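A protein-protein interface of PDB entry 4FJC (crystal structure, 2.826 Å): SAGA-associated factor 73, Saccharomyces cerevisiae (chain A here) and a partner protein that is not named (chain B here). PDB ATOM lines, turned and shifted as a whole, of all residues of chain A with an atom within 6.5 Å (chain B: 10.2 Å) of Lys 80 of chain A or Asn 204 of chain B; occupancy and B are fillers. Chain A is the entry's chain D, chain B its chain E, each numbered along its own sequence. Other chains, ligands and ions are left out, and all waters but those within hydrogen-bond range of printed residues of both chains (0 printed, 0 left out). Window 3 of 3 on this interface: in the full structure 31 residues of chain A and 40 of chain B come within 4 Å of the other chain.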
ATOM      1  N   VAL A  77      12.261   6.638 -18.728  1.00  0.00           N
ATOM      2  CA  VAL A  77      12.025   5.306 -19.322  1.00  0.00           C
ATOM      3  C   VAL A  77      13.346   4.541 -19.492  1.00  0.00           C
ATOM      4  O   VAL A  77      14.343   5.116 -19.885  1.00  0.00           O
ATOM      5  CB  VAL A  77      11.275   5.412 -20.692  1.00  0.00           C
ATOM      6  CG1 VAL A  77      10.910   4.033 -21.210  1.00  0.00           C
ATOM      7  CG2 VAL A  77      10.031   6.288 -20.573  1.00  0.00           C
ATOM      8  N   CYS A  78      13.329   3.250 -19.216  1.00  0.00           N
ATOM      9  CA  CYS A  78      14.477   2.358 -19.437  1.00  0.00           C
ATOM     10  C   CYS A  78      14.799   2.161 -20.924  1.00  0.00           C
ATOM     11  O   CYS A  78      13.900   1.861 -21.706  1.00  0.00           O
ATOM     12  CB  CYS A  78      14.156   0.991 -18.794  1.00  0.00           C
ATOM     13  SG  CYS A  78      15.404  -0.293 -18.948  1.00  0.00           S
ATOM     14  N   GLU A  79      16.062   2.320 -21.316  1.00  0.00           N
ATOM     15  CA  GLU A  79      16.466   2.180 -22.742  1.00  0.00           C
ATOM     16  C   GLU A  79      16.327   0.759 -23.267  1.00  0.00           C
ATOM     17  O   GLU A  79      16.120   0.574 -24.442  1.00  0.00           O
ATOM     18  CB  GLU A  79      17.926   2.569 -22.957  1.00  0.00           C
ATOM     19  CG  GLU A  79      18.244   4.057 -22.923  1.00  0.00           C
ATOM     20  CD  GLU A  79      17.941   4.758 -24.226  1.00  0.00           C
ATOM     21  OE1 GLU A  79      18.040   4.128 -25.291  1.00  0.00           O
ATOM     22  OE2 GLU A  79      17.595   5.953 -24.192  1.00  0.00           O
ATOM     23  N   LYS A  80      16.484  -0.238 -22.404  1.00  0.00           N
ATOM     24  CA  LYS A  80      16.398  -1.638 -22.806  1.00  0.00           C
ATOM     25  C   LYS A  80      14.990  -2.182 -22.735  1.00  0.00           C
ATOM     26  O   LYS A  80      14.476  -2.625 -23.732  1.00  0.00           O
ATOM     27  CB  LYS A  80      17.277  -2.513 -21.930  1.00  0.00           C
ATOM     28  CG  LYS A  80      17.400  -3.945 -22.440  1.00  0.00           C
ATOM     29  CD  LYS A  80      18.178  -4.853 -21.460  1.00  0.00           C
ATOM     30  CE  LYS A  80      19.345  -5.603 -22.122  1.00  0.00           C
ATOM     31  NZ  LYS A  80      19.077  -6.091 -23.512  1.00  0.00           N
ATOM     32  N   CYS A  81      14.358  -2.180 -21.562  1.00  0.00           N
ATOM     33  CA  CYS A  81      13.015  -2.794 -21.441  1.00  0.00           C
ATOM     34  C   CYS A  81      11.858  -1.865 -21.761  1.00  0.00           C
ATOM     35  O   CYS A  81      10.784  -2.343 -22.087  1.00  0.00           O
ATOM     36  CB  CYS A  81      12.799  -3.406 -20.066  1.00  0.00           C
ATOM     37  SG  CYS A  81      12.592  -2.214 -18.760  1.00  0.00           S
ATOM     38  N   GLY A  82      12.067  -0.555 -21.686  1.00  0.00           N
ATOM     39  CA  GLY A  82      11.027   0.405 -22.083  1.00  0.00           C
ATOM     40  C   GLY A  82      10.058   0.762 -20.968  1.00  0.00           C
ATOM     41  O   GLY A  82       9.103   1.484 -21.190  1.00  0.00           O
ATOM     42  N   LYS A  83      10.312   0.263 -19.766  1.00  0.00           N
ATOM     43  CA  LYS A  83       9.465   0.516 -18.621  1.00  0.00           C
ATOM     44  C   LYS A  83       9.582   1.954 -18.172  1.00  0.00           C
ATOM     45  O   LYS A  83      10.618   2.528 -18.329  1.00  0.00           O
ATOM     46  CB  LYS A  83       9.882  -0.398 -17.478  1.00  0.00           C
ATOM     47  CG  LYS A  83       9.310  -1.794 -17.621  1.00  0.00           C
ATOM     48  CD  LYS A  83       9.630  -2.630 -16.407  1.00  0.00           C
ATOM     49  CE  LYS A  83       9.188  -4.085 -16.594  1.00  0.00           C
ATOM     50  NZ  LYS A  83       9.281  -4.786 -15.275  1.00  0.00           N
ATOM     51  N   LYS B 194       1.582  -3.657 -17.159  1.00  0.00           N
ATOM     52  CA  LYS B 194       1.735  -3.595 -18.602  1.00  0.00           C
ATOM     53  C   LYS B 194       0.904  -2.472 -19.198  1.00  0.00           C
ATOM     54  O   LYS B 194       1.304  -1.829 -20.150  1.00  0.00           O
ATOM     55  CB  LYS B 194       1.308  -4.922 -19.225  1.00  0.00           C
ATOM     56  CG  LYS B 194       1.592  -5.062 -20.714  1.00  0.00           C
ATOM     57  CD  LYS B 194       3.100  -5.041 -21.000  1.00  0.00           C
ATOM     58  CE  LYS B 194       3.484  -5.758 -22.312  1.00  0.00           C
ATOM     59  NZ  LYS B 194       4.641  -5.109 -23.034  1.00  0.00           N
ATOM     60  N   HIS B 197       2.927   0.380 -18.600  1.00  0.00           N
ATOM     61  CA  HIS B 197       4.120   0.357 -19.489  1.00  0.00           C
ATOM     62  C   HIS B 197       3.751   0.861 -20.867  1.00  0.00           C
ATOM     63  O   HIS B 197       4.438   1.722 -21.427  1.00  0.00           O
ATOM     64  CB  HIS B 197       4.642  -1.070 -19.573  1.00  0.00           C
ATOM     65  CG  HIS B 197       5.983  -1.246 -20.282  1.00  0.00           C
ATOM     66  ND1 HIS B 197       6.829  -2.252 -19.963  1.00  0.00           N
ATOM     67  CD2 HIS B 197       6.588  -0.562 -21.334  1.00  0.00           C
ATOM     68  CE1 HIS B 197       7.914  -2.206 -20.751  1.00  0.00           C
ATOM     69  NE2 HIS B 197       7.774  -1.181 -21.591  1.00  0.00           N
ATOM     70  N   GLU B 198       2.641   0.370 -21.414  1.00  0.00           N
ATOM     71  CA  GLU B 198       2.242   0.754 -22.771  1.00  0.00           C
ATOM     72  C   GLU B 198       1.864   2.209 -22.853  1.00  0.00           C
ATOM     73  O   GLU B 198       2.102   2.852 -23.888  1.00  0.00           O
ATOM     74  CB  GLU B 198       1.054  -0.055 -23.284  1.00  0.00           C
ATOM     75  CG  GLU B 198       1.290  -1.543 -23.418  1.00  0.00           C
ATOM     76  CD  GLU B 198       0.081  -2.253 -23.983  1.00  0.00           C
ATOM     77  OE1 GLU B 198      -0.890  -2.525 -23.204  1.00  0.00           O
ATOM     78  OE2 GLU B 198       0.097  -2.527 -25.214  1.00  0.00           O
ATOM     79  N   LEU B 199       1.282   2.724 -21.775  1.00  0.00           N
ATOM     80  CA  LEU B 199       0.744   4.063 -21.778  1.00  0.00           C
ATOM     81  C   LEU B 199       1.776   5.145 -21.474  1.00  0.00           C
ATOM     82  O   LEU B 199       1.672   6.234 -22.008  1.00  0.00           O
ATOM     83  CB  LEU B 199      -0.450   4.170 -20.807  1.00  0.00           C
ATOM     84  CG  LEU B 199      -1.899   4.087 -21.358  1.00  0.00           C
ATOM     85  CD1 LEU B 199      -2.103   2.934 -22.321  1.00  0.00           C
ATOM     86  CD2 LEU B 199      -2.900   3.967 -20.224  1.00  0.00           C
ATOM     87  N   GLY B 201       5.416   4.551 -21.075  1.00  0.00           N
ATOM     88  CA  GLY B 201       6.736   4.247 -21.605  1.00  0.00           C
ATOM     89  C   GLY B 201       6.707   3.590 -22.965  1.00  0.00           C
ATOM     90  O   GLY B 201       5.739   3.738 -23.718  1.00  0.00           O
ATOM     91  N   ALA B 202       7.758   2.832 -23.268  1.00  0.00           N
ATOM     92  CA  ALA B 202       8.029   2.358 -24.635  1.00  0.00           C
ATOM     93  C   ALA B 202       7.698   0.887 -24.878  1.00  0.00           C
ATOM     94  O   ALA B 202       8.069   0.001 -24.103  1.00  0.00           O
ATOM     95  CB  ALA B 202       9.485   2.622 -24.988  1.00  0.00           C
ATOM     96  N   LEU B 203       7.024   0.658 -26.001  1.00  0.00           N
ATOM     97  CA  LEU B 203       6.578  -0.685 -26.449  1.00  0.00           C
ATOM     98  C   LEU B 203       7.724  -1.662 -26.730  1.00  0.00           C
ATOM     99  O   LEU B 203       7.627  -2.836 -26.360  1.00  0.00           O
ATOM    100  CB  LEU B 203       5.661  -0.602 -27.701  1.00  0.00           C
ATOM    101  CG  LEU B 203       5.462   0.649 -28.601  1.00  0.00           C
ATOM    102  CD1 LEU B 203       4.503   1.652 -27.942  1.00  0.00           C
ATOM    103  CD2 LEU B 203       6.775   1.310 -29.040  1.00  0.00           C
ATOM    104  N   ASN B 204       8.779  -1.153 -27.381  1.00  0.00           N
ATOM    105  CA  ASN B 204       9.991  -1.904 -27.792  1.00  0.00           C
ATOM    106  C   ASN B 204      10.186  -1.777 -29.303  1.00  0.00           C
ATOM    107  O   ASN B 204      10.257  -2.777 -30.017  1.00  0.00           O
ATOM    108  CB  ASN B 204       9.989  -3.406 -27.387  1.00  0.00           C
ATOM    109  CG  ASN B 204      10.273  -3.632 -25.898  1.00  0.00           C
ATOM    110  OD1 ASN B 204      11.097  -2.939 -25.285  1.00  0.00           O
ATOM    111  ND2 ASN B 204       9.598  -4.621 -25.319  1.00  0.00           N
ATOM    112  N   ASN B 216       1.220   3.090 -26.981  1.00  0.00           N
ATOM    113  CA  ASN B 216      -0.167   2.897 -26.549  1.00  0.00           C
ATOM    114  C   ASN B 216      -0.854   1.777 -27.327  1.00  0.00           C
ATOM    115  O   ASN B 216      -1.087   1.896 -28.536  1.00  0.00           O
ATOM    116  CB  ASN B 216      -0.977   4.196 -26.692  1.00  0.00           C
ATOM    117  CG  ASN B 216      -0.957   4.751 -28.108  1.00  0.00           C
ATOM    118  OD1 ASN B 216       0.079   4.739 -28.777  1.00  0.00           O
ATOM    119  ND2 ASN B 216      -2.104   5.233 -28.572  1.00  0.00           N
ATOM    120  N   ARG B 217      -1.169   0.686 -26.645  1.00  0.00           N
ATOM    121  CA  ARG B 217      -1.827  -0.431 -27.284  1.00  0.00           C
ATOM    122  C   ARG B 217      -2.742  -1.069 -26.259  1.00  0.00           C
ATOM    123  O   ARG B 217      -2.917  -0.565 -25.141  1.00  0.00           O
ATOM    124  CB  ARG B 217      -0.792  -1.450 -27.812  1.00  0.00           C
ATOM    125  CG  ARG B 217       0.102  -0.996 -28.975  1.00  0.00           C
ATOM    126  CD  ARG B 217      -0.419  -1.421 -30.340  1.00  0.00           C
ATOM    127  NE  ARG B 217      -0.179  -0.374 -31.333  1.00  0.00           N
ATOM    128  CZ  ARG B 217      -1.010   0.642 -31.592  1.00  0.00           C
ATOM    129  NH1 ARG B 217      -2.173   0.771 -30.943  1.00  0.00           N
ATOM    130  NH2 ARG B 217      -0.682   1.541 -32.518  1.00  0.00           N
ATOM    131  N   THR B 219      -2.590  -4.418 -25.380  1.00  0.00           N
ATOM    132  CA  THR B 219      -2.086  -5.698 -24.891  1.00  0.00           C
ATOM    133  C   THR B 219      -2.324  -5.874 -23.405  1.00  0.00           C
ATOM    134  O   THR B 219      -2.762  -6.936 -22.972  1.00  0.00           O
ATOM    135  CB  THR B 219      -0.611  -5.871 -25.211  1.00  0.00           C
ATOM    136  OG1 THR B 219      -0.491  -5.892 -26.624  1.00  0.00           O
ATOM    137  CG2 THR B 219      -0.079  -7.171 -24.642  1.00  0.00           C
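NE2 of His 197 of chain B is in hydrogen-bond range of N of Lys 83 of chain A, 3.4 Å away.
A ring nitrogen (NE2) of His 197 of chain B sits close to the backbone carbonyl oxygen (O) of Cys 81 of chain A.
N of Ala 202 of chain B is in hydrogen-bond range of O of Gly 82 of chain A, 2.8 Å away.
A ring nitrogen (NE2) of His 197 of chain B sits at hydrogen-bond distance from the backbone carbonyl oxygen (O) of Gly 82 of chain A, 3.0 Å away.
The backbone carbonyl oxygen (O) of Cys 81 of chain A sits close to the side-chain amide oxygen (OD1) of Asn 204 of chain B (3.3 Å).
The side-chain sulfur of Cys 81 of chain A lies close to the backbone NH of Lys 83 of chain A, at 3.5 Å.
A ring nitrogen (NE2) of His 197 of chain B lies within hydrogen-bond range of the backbone carbonyl oxygen (O) of Ala 202 of chain B (2.8 Å).
The backbone NH (N) of Cys 78 of chain A lies within hydrogen-bond range of the backbone carbonyl oxygen (O) of Lys 83 of chain A, 2.9 Å away.
The side-chain sulfur (SG) of Cys 78 of chain A lies close to the backbone NH (N) of Lys 80 of chain A (3.6 Å).
Ala 202 of chain B touches Val 77 of chain A (N to CG1, 3.95 Å).
Lys 80 of chain A touches Asn 204 of chain B (O to OD1, 3.7 Å).
Gly 201 of chain B touches Gly 82 of chain A (C to O, 3.7 Å).
No residue of chain B comes within 4 Å of Cys 78 of chain A.
Of chain B, only Asn 204 comes within 4 Å of Lys 80 of chain A.
Of the printed residues of chain B, Lys 83 of chain A touches His 197.
Of the printed residues of chain A, Ala 202 of chain B touches Val 77 (3.95 Å) and Gly 82 (2.8 Å).
Of chain A, only Lys 80 (3.7 Å) and Cys 81 (3.3 Å) come within 4 Å of Asn 204 of chain B.
The nearest residue of chain B that does not touch Lys 80 of chain A is Ala 202 of chain B (6.9 Å).
The nearest residue of chain A that does not touch Asn 204 of chain B is Gly 82 of chain A (4.4 Å).
The nearest printed residue of chain B that does not touch Lys 83 of chain A is Ala 202 of chain B (4.9 Å).
Hydrophobic or aromatic side chains of chain B within 4 Å of the printed part of chain A: His 197 and Ala 202.
Printed residues of chain A that touch a printed residue of chain B: Val 77, Lys 80, Cys 81, Gly 82 and Lys 83.
Hydrophobic or aromatic side chains of chain A that line the printed part of chain B: Val 77.
Among the printed residues, no Asp or Glu carboxylate lies within 4 Å of a Lys or Arg side-chain nitrogen of the other chain.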
